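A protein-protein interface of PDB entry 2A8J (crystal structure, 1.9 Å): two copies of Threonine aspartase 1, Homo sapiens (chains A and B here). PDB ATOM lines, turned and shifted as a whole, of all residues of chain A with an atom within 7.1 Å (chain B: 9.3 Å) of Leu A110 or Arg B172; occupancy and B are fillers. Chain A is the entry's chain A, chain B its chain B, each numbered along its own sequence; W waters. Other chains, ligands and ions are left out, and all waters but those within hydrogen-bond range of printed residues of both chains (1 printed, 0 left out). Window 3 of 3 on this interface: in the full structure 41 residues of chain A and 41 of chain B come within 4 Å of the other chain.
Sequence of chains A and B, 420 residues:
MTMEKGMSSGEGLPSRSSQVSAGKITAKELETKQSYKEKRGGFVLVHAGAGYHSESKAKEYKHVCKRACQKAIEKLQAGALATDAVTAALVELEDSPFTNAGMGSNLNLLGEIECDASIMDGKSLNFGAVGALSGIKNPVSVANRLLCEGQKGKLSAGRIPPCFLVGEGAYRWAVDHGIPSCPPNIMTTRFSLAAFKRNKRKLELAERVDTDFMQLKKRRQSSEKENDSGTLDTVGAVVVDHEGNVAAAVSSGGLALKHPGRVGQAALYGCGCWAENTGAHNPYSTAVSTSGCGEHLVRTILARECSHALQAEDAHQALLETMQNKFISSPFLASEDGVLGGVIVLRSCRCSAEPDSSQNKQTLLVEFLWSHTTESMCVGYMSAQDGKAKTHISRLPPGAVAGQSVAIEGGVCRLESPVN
Water W1 bridges a ring nitrogen (NE2) of His A259 (3.0 Å) and the side-chain carboxylate (OD2) of Asp B176 (3.0 Å).
OD2 of Asp B176 lies within salt-bridge range of NE of Arg B172 (3.7 Å).
N of Leu A109 sits close to O of Leu A257.
O of Trp B173 sits at hydrogen-bond distance from ND1 of His B177, at 2.8 Å.
The backbone NH (N) of Leu A109 lies within hydrogen-bond range of the backbone carbonyl oxygen (O) of Lys A258, at 2.7 Å.
The backbone NH (N) of Leu A110 lies within hydrogen-bond range of the side-chain amide oxygen (OD1) of Asn A108 (2.8 Å).
Arg B172 touches Leu A109.
Leu A110 touches Arg B172.
CE1 of His A259 touches O of Gly B169, at 3.0 Å.
His A259 touches Arg B172 (NE2 to CD, 3.9 Å).
CD1 of Trp B173 touches CD2 of His A259 (3.6 Å).
Pro A260 touches Gly B169.
Arg B172 touches Pro A260 (NH1 to CD, 3.5 Å).
Hydrophobic or aromatic side chains of chain A that line the printed part of chain B: Leu A109, Leu A110, His A259 and Pro A260.
Of the 23 printed residues of chain B, 3 touch a printed residue of chain A.
Hydrophobic or aromatic side chains of chain B within 4 Å of the printed part of chain A: Trp B173.
Among the printed residues, no Asp or Glu carboxylate lies within 4 Å of a Lys or Arg side-chain nitrogen of the other chain.
Of the printed residues of chain A, Arg B172 touches Leu A109 (3.5 Å), Leu A110 (3.996 Å), His A259 (3.9 Å) and Pro A260 (3.5 Å).
No residue of chain B comes within 4 Å of Asn A108.
No residue of chain B comes within 4 Å of Gly A111.
Printed residues of chain A within 4 Å of Trp B173: His A259 (3.6 Å).
Printed residues of chain B within 4 Å of His A259: Gly B169, Arg B172 and Trp B173.
Of the printed residues of chain B, Pro A260 touches Gly B169 and Arg B172.
The nearest printed residue of chain A that does not touch Arg B172 is Lys A258 (6.8 Å).
The nearest printed residue of chain B that does not touch His A259 is Leu B165 (4.4 Å).
No position is printed for both chains.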
ATOM      1  N   LEU A 107      20.468 -33.713  13.345  1.00  0.00           N
ATOM      2  CA  LEU A 107      19.257 -32.912  13.473  1.00  0.00           C
ATOM      3  C   LEU A 107      18.787 -32.982  14.927  1.00  0.00           C
ATOM      4  O   LEU A 107      18.900 -34.032  15.559  1.00  0.00           O
ATOM      5  CB  LEU A 107      18.160 -33.461  12.560  1.00  0.00           C
ATOM      6  CG  LEU A 107      18.405 -33.541  11.048  1.00  0.00           C
ATOM      7  CD1 LEU A 107      19.616 -34.427  10.747  1.00  0.00           C
ATOM      8  CD2 LEU A 107      17.158 -34.119  10.383  1.00  0.00           C
ATOM      9  N   ASN A 108      18.278 -31.873  15.461  1.00  0.00           N
ATOM     10  CA  ASN A 108      17.792 -31.867  16.839  1.00  0.00           C
ATOM     11  C   ASN A 108      16.353 -32.381  16.903  1.00  0.00           C
ATOM     12  O   ASN A 108      15.790 -32.794  15.884  1.00  0.00           O
ATOM     13  CB  ASN A 108      17.877 -30.460  17.452  1.00  0.00           C
ATOM     14  CG  ASN A 108      16.867 -29.486  16.864  1.00  0.00           C
ATOM     15  OD1 ASN A 108      15.974 -29.865  16.099  1.00  0.00           O
ATOM     16  ND2 ASN A 108      17.005 -28.212  17.228  1.00  0.00           N
ATOM     17  N   LEU A 109      15.766 -32.351  18.095  1.00  0.00           N
ATOM     18  CA  LEU A 109      14.396 -32.823  18.302  1.00  0.00           C
ATOM     19  C   LEU A 109      13.417 -32.349  17.241  1.00  0.00           C
ATOM     20  O   LEU A 109      12.537 -33.100  16.822  1.00  0.00           O
ATOM     21  CB  LEU A 109      13.885 -32.386  19.676  1.00  0.00           C
ATOM     22  CG  LEU A 109      12.462 -32.847  19.995  1.00  0.00           C
ATOM     23  CD1 LEU A 109      12.429 -34.367  20.088  1.00  0.00           C
ATOM     24  CD2 LEU A 109      11.996 -32.218  21.294  1.00  0.00           C
ATOM     25  N   LEU A 110      13.565 -31.102  16.810  1.00  0.00           N
ATOM     26  CA  LEU A 110      12.681 -30.530  15.800  1.00  0.00           C
ATOM     27  C   LEU A 110      13.168 -30.744  14.359  1.00  0.00           C
ATOM     28  O   LEU A 110      12.651 -30.128  13.429  1.00  0.00           O
ATOM     29  CB  LEU A 110      12.495 -29.030  16.062  1.00  0.00           C
ATOM     30  CG  LEU A 110      11.814 -28.633  17.375  1.00  0.00           C
ATOM     31  CD1 LEU A 110      11.792 -27.118  17.496  1.00  0.00           C
ATOM     32  CD2 LEU A 110      10.394 -29.193  17.409  1.00  0.00           C
ATOM     33  N   GLY A 111      14.150 -31.621  14.176  1.00  0.00           N
ATOM     34  CA  GLY A 111      14.676 -31.870  12.843  1.00  0.00           C
ATOM     35  C   GLY A 111      15.438 -30.665  12.315  1.00  0.00           C
ATOM     36  O   GLY A 111      15.588 -30.490  11.102  1.00  0.00           O
ATOM     37  N   GLU A 112      15.921 -29.835  13.236  1.00  0.00           N
ATOM     38  CA  GLU A 112      16.671 -28.630  12.886  1.00  0.00           C
ATOM     39  C   GLU A 112      18.142 -28.788  13.271  1.00  0.00           C
ATOM     40  O   GLU A 112      18.485 -29.578  14.151  1.00  0.00           O
ATOM     41  CB  GLU A 112      16.093 -27.416  13.615  1.00  0.00           C
ATOM     42  CG  GLU A 112      14.606 -27.172  13.402  1.00  0.00           C
ATOM     43  CD  GLU A 112      14.305 -26.477  12.097  1.00  0.00           C
ATOM     44  OE1 GLU A 112      14.950 -25.444  11.811  1.00  0.00           O
ATOM     45  OE2 GLU A 112      13.417 -26.954  11.358  1.00  0.00           O
ATOM     46  N   ILE A 113      19.004 -28.026  12.609  1.00  0.00           N
ATOM     47  CA  ILE A 113      20.434 -28.071  12.879  1.00  0.00           C
ATOM     48  C   ILE A 113      20.843 -26.905  13.780  1.00  0.00           C
ATOM     49  O   ILE A 113      20.444 -25.768  13.555  1.00  0.00           O
ATOM     50  CB  ILE A 113      21.241 -28.016  11.557  1.00  0.00           C
ATOM     51  CG1 ILE A 113      21.016 -29.309  10.765  1.00  0.00           C
ATOM     52  CG2 ILE A 113      22.718 -27.823  11.843  1.00  0.00           C
ATOM     53  CD1 ILE A 113      21.655 -29.312   9.390  1.00  0.00           C
ATOM     54  N   LEU A 257      18.818 -35.446  17.955  1.00  0.00           N
ATOM     55  CA  LEU A 257      17.528 -35.259  18.609  1.00  0.00           C
ATOM     56  C   LEU A 257      17.551 -34.442  19.897  1.00  0.00           C
ATOM     57  O   LEU A 257      16.565 -34.412  20.638  1.00  0.00           O
ATOM     58  CB  LEU A 257      16.860 -36.615  18.868  1.00  0.00           C
ATOM     59  CG  LEU A 257      16.478 -37.401  17.613  1.00  0.00           C
ATOM     60  CD1 LEU A 257      15.644 -38.609  18.015  1.00  0.00           C
ATOM     61  CD2 LEU A 257      15.681 -36.515  16.658  1.00  0.00           C
ATOM     62  N   LYS A 258      18.667 -33.764  20.158  1.00  0.00           N
ATOM     63  CA  LYS A 258      18.781 -32.936  21.355  1.00  0.00           C
ATOM     64  C   LYS A 258      17.654 -31.921  21.375  1.00  0.00           C
ATOM     65  O   LYS A 258      17.127 -31.544  20.326  1.00  0.00           O
ATOM     66  CB  LYS A 258      20.113 -32.183  21.357  1.00  0.00           C
ATOM     67  CG  LYS A 258      20.205 -31.120  20.258  1.00  0.00           C
ATOM     68  CD  LYS A 258      21.644 -30.679  20.035  1.00  0.00           C
ATOM     69  CE  LYS A 258      21.735 -29.540  19.025  1.00  0.00           C
ATOM     70  NZ  LYS A 258      23.144 -29.115  18.819  1.00  0.00           N
ATOM     71  N   HIS A 259      17.291 -31.470  22.571  1.00  0.00           N
ATOM     72  CA  HIS A 259      16.240 -30.478  22.710  1.00  0.00           C
ATOM     73  C   HIS A 259      16.787 -29.191  22.107  1.00  0.00           C
ATOM     74  O   HIS A 259      17.990 -28.932  22.186  1.00  0.00           O
ATOM     75  CB  HIS A 259      15.903 -30.254  24.192  1.00  0.00           C
ATOM     76  CG  HIS A 259      14.785 -29.283  24.418  1.00  0.00           C
ATOM     77  ND1 HIS A 259      14.923 -27.926  24.211  1.00  0.00           N
ATOM     78  CD2 HIS A 259      13.491 -29.478  24.778  1.00  0.00           C
ATOM     79  CE1 HIS A 259      13.764 -27.328  24.430  1.00  0.00           C
ATOM     80  NE2 HIS A 259      12.878 -28.247  24.773  1.00  0.00           N
ATOM     81  N   PRO A 260      15.923 -28.390  21.466  1.00  0.00           N
ATOM     82  CA  PRO A 260      16.349 -27.126  20.857  1.00  0.00           C
ATOM     83  C   PRO A 260      17.037 -26.230  21.893  1.00  0.00           C
ATOM     84  O   PRO A 260      16.573 -26.124  23.025  1.00  0.00           O
ATOM     85  CB  PRO A 260      15.036 -26.508  20.376  1.00  0.00           C
ATOM     86  CG  PRO A 260      14.174 -27.707  20.081  1.00  0.00           C
ATOM     87  CD  PRO A 260      14.484 -28.629  21.237  1.00  0.00           C
ATOM     88  N   VAL B 130      21.041 -21.303  31.877  1.00  0.00           N
ATOM     89  CA  VAL B 130      20.282 -20.794  30.742  1.00  0.00           C
ATOM     90  C   VAL B 130      20.984 -19.552  30.203  1.00  0.00           C
ATOM     91  O   VAL B 130      21.493 -18.741  30.968  1.00  0.00           O
ATOM     92  CB  VAL B 130      18.830 -20.417  31.133  1.00  0.00           C
ATOM     93  CG1 VAL B 130      18.033 -21.686  31.436  1.00  0.00           C
ATOM     94  CG2 VAL B 130      18.832 -19.478  32.329  1.00  0.00           C
ATOM     95  N   LEU B 133      18.040 -15.949  27.542  1.00  0.00           N
ATOM     96  CA  LEU B 133      16.650 -16.318  27.771  1.00  0.00           C
ATOM     97  C   LEU B 133      15.743 -15.099  27.944  1.00  0.00           C
ATOM     98  O   LEU B 133      16.023 -14.216  28.756  1.00  0.00           O
ATOM     99  CB  LEU B 133      16.547 -17.199  29.023  1.00  0.00           C
ATOM    100  CG  LEU B 133      15.147 -17.631  29.491  1.00  0.00           C
ATOM    101  CD1 LEU B 133      14.500 -18.530  28.433  1.00  0.00           C
ATOM    102  CD2 LEU B 133      15.266 -18.372  30.824  1.00  0.00           C
ATOM    103  N   SER B 134      14.665 -15.045  27.168  1.00  0.00           N
ATOM    104  CA  SER B 134      13.697 -13.953  27.285  1.00  0.00           C
ATOM    105  C   SER B 134      12.294 -14.551  27.439  1.00  0.00           C
ATOM    106  O   SER B 134      12.092 -15.739  27.186  1.00  0.00           O
ATOM    107  CB  SER B 134      13.753 -13.034  26.060  1.00  0.00           C
ATOM    108  OG  SER B 134      13.644 -13.761  24.859  1.00  0.00           O
ATOM    109  N   GLY B 135      11.340 -13.737  27.880  1.00  0.00           N
ATOM    110  CA  GLY B 135       9.980 -14.222  28.047  1.00  0.00           C
ATOM    111  C   GLY B 135       9.697 -14.952  29.351  1.00  0.00           C
ATOM    112  O   GLY B 135       8.549 -15.323  29.612  1.00  0.00           O
ATOM    113  N   ILE B 136      10.731 -15.171  30.163  1.00  0.00           N
ATOM    114  CA  ILE B 136      10.582 -15.854  31.451  1.00  0.00           C
ATOM    115  C   ILE B 136      10.831 -14.865  32.600  1.00  0.00           C
ATOM    116  O   ILE B 136      11.824 -14.132  32.602  1.00  0.00           O
ATOM    117  CB  ILE B 136      11.578 -17.028  31.573  1.00  0.00           C
ATOM    118  CG1 ILE B 136      11.354 -18.029  30.438  1.00  0.00           C
ATOM    119  CG2 ILE B 136      11.422 -17.708  32.934  1.00  0.00           C
ATOM    120  CD1 ILE B 136       9.986 -18.708  30.450  1.00  0.00           C
ATOM    121  N   VAL B 142      14.543 -21.539  35.887  1.00  0.00           N
ATOM    122  CA  VAL B 142      14.771 -22.472  34.796  1.00  0.00           C
ATOM    123  C   VAL B 142      16.076 -23.216  35.024  1.00  0.00           C
ATOM    124  O   VAL B 142      16.158 -24.426  34.817  1.00  0.00           O
ATOM    125  CB  VAL B 142      14.840 -21.739  33.436  1.00  0.00           C
ATOM    126  CG1 VAL B 142      14.825 -22.749  32.299  1.00  0.00           C
ATOM    127  CG2 VAL B 142      13.681 -20.765  33.313  1.00  0.00           C
ATOM    128  N   LEU B 146      16.481 -27.227  35.493  1.00  0.00           N
ATOM    129  CA  LEU B 146      17.356 -28.003  34.627  1.00  0.00           C
ATOM    130  C   LEU B 146      18.251 -28.878  35.491  1.00  0.00           C
ATOM    131  O   LEU B 146      18.524 -30.034  35.158  1.00  0.00           O
ATOM    132  CB  LEU B 146      18.206 -27.074  33.754  1.00  0.00           C
ATOM    133  CG  LEU B 146      17.549 -26.523  32.486  1.00  0.00           C
ATOM    134  CD1 LEU B 146      18.384 -25.377  31.926  1.00  0.00           C
ATOM    135  CD2 LEU B 146      17.409 -27.633  31.455  1.00  0.00           C
ATOM    136  N   LEU B 165      20.790 -24.669  28.297  1.00  0.00           N
ATOM    137  CA  LEU B 165      19.890 -24.346  27.184  1.00  0.00           C
ATOM    138  C   LEU B 165      19.923 -22.835  26.914  1.00  0.00           C
ATOM    139  O   LEU B 165      20.102 -22.036  27.841  1.00  0.00           O
ATOM    140  CB  LEU B 165      18.440 -24.741  27.515  1.00  0.00           C
ATOM    141  CG  LEU B 165      18.076 -26.214  27.709  1.00  0.00           C
ATOM    142  CD1 LEU B 165      16.572 -26.344  27.914  1.00  0.00           C
ATOM    143  CD2 LEU B 165      18.516 -27.010  26.487  1.00  0.00           C
ATOM    144  N   VAL B 166      19.741 -22.443  25.655  1.00  0.00           N
ATOM    145  CA  VAL B 166      19.733 -21.021  25.307  1.00  0.00           C
ATOM    146  C   VAL B 166      18.573 -20.634  24.388  1.00  0.00           C
ATOM    147  O   VAL B 166      17.904 -21.490  23.811  1.00  0.00           O
ATOM    148  CB  VAL B 166      21.062 -20.583  24.609  1.00  0.00           C
ATOM    149  CG1 VAL B 166      22.256 -20.931  25.487  1.00  0.00           C
ATOM    150  CG2 VAL B 166      21.187 -21.238  23.256  1.00  0.00           C
ATOM    151  N   GLY B 167      18.360 -19.329  24.261  1.00  0.00           N
ATOM    152  CA  GLY B 167      17.325 -18.794  23.392  1.00  0.00           C
ATOM    153  C   GLY B 167      15.935 -19.401  23.454  1.00  0.00           C
ATOM    154  O   GLY B 167      15.459 -19.820  24.506  1.00  0.00           O
ATOM    155  N   GLU B 168      15.279 -19.421  22.299  1.00  0.00           N
ATOM    156  CA  GLU B 168      13.929 -19.957  22.148  1.00  0.00           C
ATOM    157  C   GLU B 168      13.825 -21.367  22.723  1.00  0.00           C
ATOM    158  O   GLU B 168      12.846 -21.707  23.382  1.00  0.00           O
ATOM    159  CB  GLU B 168      13.561 -19.976  20.667  1.00  0.00           C
ATOM    160  CG  GLU B 168      13.712 -18.622  19.990  1.00  0.00           C
ATOM    161  CD  GLU B 168      13.880 -18.736  18.486  1.00  0.00           C
ATOM    162  OE1 GLU B 168      13.089 -19.470  17.852  1.00  0.00           O
ATOM    163  OE2 GLU B 168      14.803 -18.090  17.935  1.00  0.00           O
ATOM    164  N   GLY B 169      14.838 -22.185  22.468  1.00  0.00           N
ATOM    165  CA  GLY B 169      14.832 -23.540  22.984  1.00  0.00           C
ATOM    166  C   GLY B 169      14.731 -23.560  24.501  1.00  0.00           C
ATOM    167  O   GLY B 169      14.068 -24.435  25.071  1.00  0.00           O
ATOM    168  N   ALA B 170      15.396 -22.602  25.150  1.00  0.00           N
ATOM    169  CA  ALA B 170      15.388 -22.490  26.610  1.00  0.00           C
ATOM    170  C   ALA B 170      13.991 -22.072  27.061  1.00  0.00           C
ATOM    171  O   ALA B 170      13.447 -22.594  28.035  1.00  0.00           O
ATOM    172  CB  ALA B 170      16.419 -21.457  27.057  1.00  0.00           C
ATOM    173  N   TYR B 171      13.419 -21.120  26.336  1.00  0.00           N
ATOM    174  CA  TYR B 171      12.085 -20.631  26.629  1.00  0.00           C
ATOM    175  C   TYR B 171      11.068 -21.775  26.519  1.00  0.00           C
ATOM    176  O   TYR B 171      10.241 -21.975  27.410  1.00  0.00           O
ATOM    177  CB  TYR B 171      11.719 -19.520  25.647  1.00  0.00           C
ATOM    178  CG  TYR B 171      10.271 -19.116  25.717  1.00  0.00           C
ATOM    179  CD1 TYR B 171       9.803 -18.300  26.745  1.00  0.00           C
ATOM    180  CD2 TYR B 171       9.353 -19.584  24.774  1.00  0.00           C
ATOM    181  CE1 TYR B 171       8.460 -17.961  26.836  1.00  0.00           C
ATOM    182  CE2 TYR B 171       8.009 -19.253  24.858  1.00  0.00           C
ATOM    183  CZ  TYR B 171       7.569 -18.445  25.887  1.00  0.00           C
ATOM    184  OH  TYR B 171       6.233 -18.130  25.975  1.00  0.00           O
ATOM    185  N   ARG B 172      11.140 -22.523  25.422  1.00  0.00           N
ATOM    186  CA  ARG B 172      10.226 -23.643  25.192  1.00  0.00           C
ATOM    187  C   ARG B 172      10.334 -24.679  26.307  1.00  0.00           C
ATOM    188  O   ARG B 172       9.322 -25.163  26.818  1.00  0.00           O
ATOM    189  CB  ARG B 172      10.535 -24.313  23.846  1.00  0.00           C
ATOM    190  CG  ARG B 172       9.587 -25.456  23.486  1.00  0.00           C
ATOM    191  CD  ARG B 172      10.212 -26.435  22.492  1.00  0.00           C
ATOM    192  NE  ARG B 172       9.307 -27.541  22.182  1.00  0.00           N
ATOM    193  CZ  ARG B 172       9.688 -28.697  21.643  1.00  0.00           C
ATOM    194  NH1 ARG B 172      10.966 -28.906  21.353  1.00  0.00           N
ATOM    195  NH2 ARG B 172       8.793 -29.646  21.392  1.00  0.00           N
ATOM    196  N   TRP B 173      11.567 -25.025  26.676  1.00  0.00           N
ATOM    197  CA  TRP B 173      11.794 -26.011  27.727  1.00  0.00           C
ATOM    198  C   TRP B 173      11.168 -25.506  29.031  1.00  0.00           C
ATOM    199  O   TRP B 173      10.542 -26.266  29.774  1.00  0.00           O
ATOM    200  CB  TRP B 173      13.296 -26.245  27.911  1.00  0.00           C
ATOM    201  CG  TRP B 173      13.652 -27.440  28.751  1.00  0.00           C
ATOM    202  CD1 TRP B 173      13.895 -28.713  28.311  1.00  0.00           C
ATOM    203  CD2 TRP B 173      13.769 -27.479  30.176  1.00  0.00           C
ATOM    204  NE1 TRP B 173      14.155 -29.545  29.380  1.00  0.00           N
ATOM    205  CE2 TRP B 173      14.084 -28.809  30.536  1.00  0.00           C
ATOM    206  CE3 TRP B 173      13.640 -26.516  31.188  1.00  0.00           C
ATOM    207  CZ2 TRP B 173      14.263 -29.203  31.868  1.00  0.00           C
ATOM    208  CZ3 TRP B 173      13.820 -26.909  32.518  1.00  0.00           C
ATOM    209  CH2 TRP B 173      14.129 -28.238  32.842  1.00  0.00           C
ATOM    210  N   ALA B 174      11.325 -24.212  29.285  1.00  0.00           N
ATOM    211  CA  ALA B 174      10.784 -23.588  30.488  1.00  0.00           C
ATOM    212  C   ALA B 174       9.266 -23.760  30.578  1.00  0.00           C
ATOM    213  O   ALA B 174       8.745 -24.328  31.540  1.00  0.00           O
ATOM    214  CB  ALA B 174      11.149 -22.097  30.510  1.00  0.00           C
ATOM    215  N   VAL B 175       8.567 -23.260  29.565  1.00  0.00           N
ATOM    216  CA  VAL B 175       7.114 -23.340  29.508  1.00  0.00           C
ATOM    217  C   VAL B 175       6.600 -24.772  29.588  1.00  0.00           C
ATOM    218  O   VAL B 175       5.605 -25.041  30.262  1.00  0.00           O
ATOM    219  CB  VAL B 175       6.587 -22.675  28.219  1.00  0.00           C
ATOM    220  CG1 VAL B 175       5.111 -22.973  28.034  1.00  0.00           C
ATOM    221  CG2 VAL B 175       6.812 -21.175  28.293  1.00  0.00           C
ATOM    222  N   ASP B 176       7.276 -25.693  28.906  1.00  0.00           N
ATOM    223  CA  ASP B 176       6.860 -27.091  28.917  1.00  0.00           C
ATOM    224  C   ASP B 176       7.139 -27.769  30.249  1.00  0.00           C
ATOM    225  O   ASP B 176       6.791 -28.934  30.441  1.00  0.00           O
ATOM    226  CB  ASP B 176       7.541 -27.872  27.790  1.00  0.00           C
ATOM    227  CG  ASP B 176       7.021 -27.486  26.417  1.00  0.00           C
ATOM    228  OD1 ASP B 176       5.787 -27.469  26.239  1.00  0.00           O
ATOM    229  OD2 ASP B 176       7.839 -27.203  25.514  1.00  0.00           O
ATOM    230  N   HIS B 177       7.774 -27.047  31.166  1.00  0.00           N
ATOM    231  CA  HIS B 177       8.072 -27.599  32.480  1.00  0.00           C
ATOM    232  C   HIS B 177       7.394 -26.812  33.595  1.00  0.00           C
ATOM    233  O   HIS B 177       7.780 -26.905  34.762  1.00  0.00           O
ATOM    234  CB  HIS B 177       9.580 -27.667  32.713  1.00  0.00           C
ATOM    235  CG  HIS B 177      10.231 -28.834  32.041  1.00  0.00           C
ATOM    236  ND1 HIS B 177      10.355 -28.931  30.673  1.00  0.00           N
ATOM    237  CD2 HIS B 177      10.737 -29.983  32.546  1.00  0.00           C
ATOM    238  CE1 HIS B 177      10.908 -30.089  30.364  1.00  0.00           C
ATOM    239  NE2 HIS B 177      11.148 -30.747  31.483  1.00  0.00           N
ATOM    240  N   GLY B 178       6.382 -26.035  33.217  1.00  0.00           N
ATOM    241  CA  GLY B 178       5.624 -25.266  34.186  1.00  0.00           C
ATOM    242  C   GLY B 178       6.192 -23.960  34.706  1.00  0.00           C
ATOM    243  O   GLY B 178       5.687 -23.429  35.695  1.00  0.00           O
ATOM    244  N   ILE B 179       7.225 -23.427  34.066  1.00  0.00           N
ATOM    245  CA  ILE B 179       7.791 -22.165  34.529  1.00  0.00           C
ATOM    246  C   ILE B 179       7.020 -21.002  33.906  1.00  0.00           C
ATOM    247  O   ILE B 179       6.863 -20.927  32.688  1.00  0.00           O
ATOM    248  CB  ILE B 179       9.284 -22.052  34.172  1.00  0.00           C
ATOM    249  CG1 ILE B 179      10.040 -23.243  34.763  1.00  0.00           C
ATOM    250  CG2 ILE B 179       9.847 -20.750  34.717  1.00  0.00           C
ATOM    251  CD1 ILE B 179      11.510 -23.285  34.415  1.00  0.00           C
ATOM    252  N   SER B 181       5.835 -17.494  32.365  1.00  0.00           N
ATOM    253  CA  SER B 181       6.376 -16.512  31.440  1.00  0.00           C
ATOM    254  C   SER B 181       5.920 -15.122  31.871  1.00  0.00           C
ATOM    255  O   SER B 181       5.109 -14.989  32.788  1.00  0.00           O
ATOM    256  CB  SER B 181       5.891 -16.814  30.022  1.00  0.00           C
ATOM    257  OG  SER B 181       4.491 -17.011  29.998  1.00  0.00           O
HETATM  258  O   HOH W   1      10.244 -29.007  26.027  1.00  0.00           O
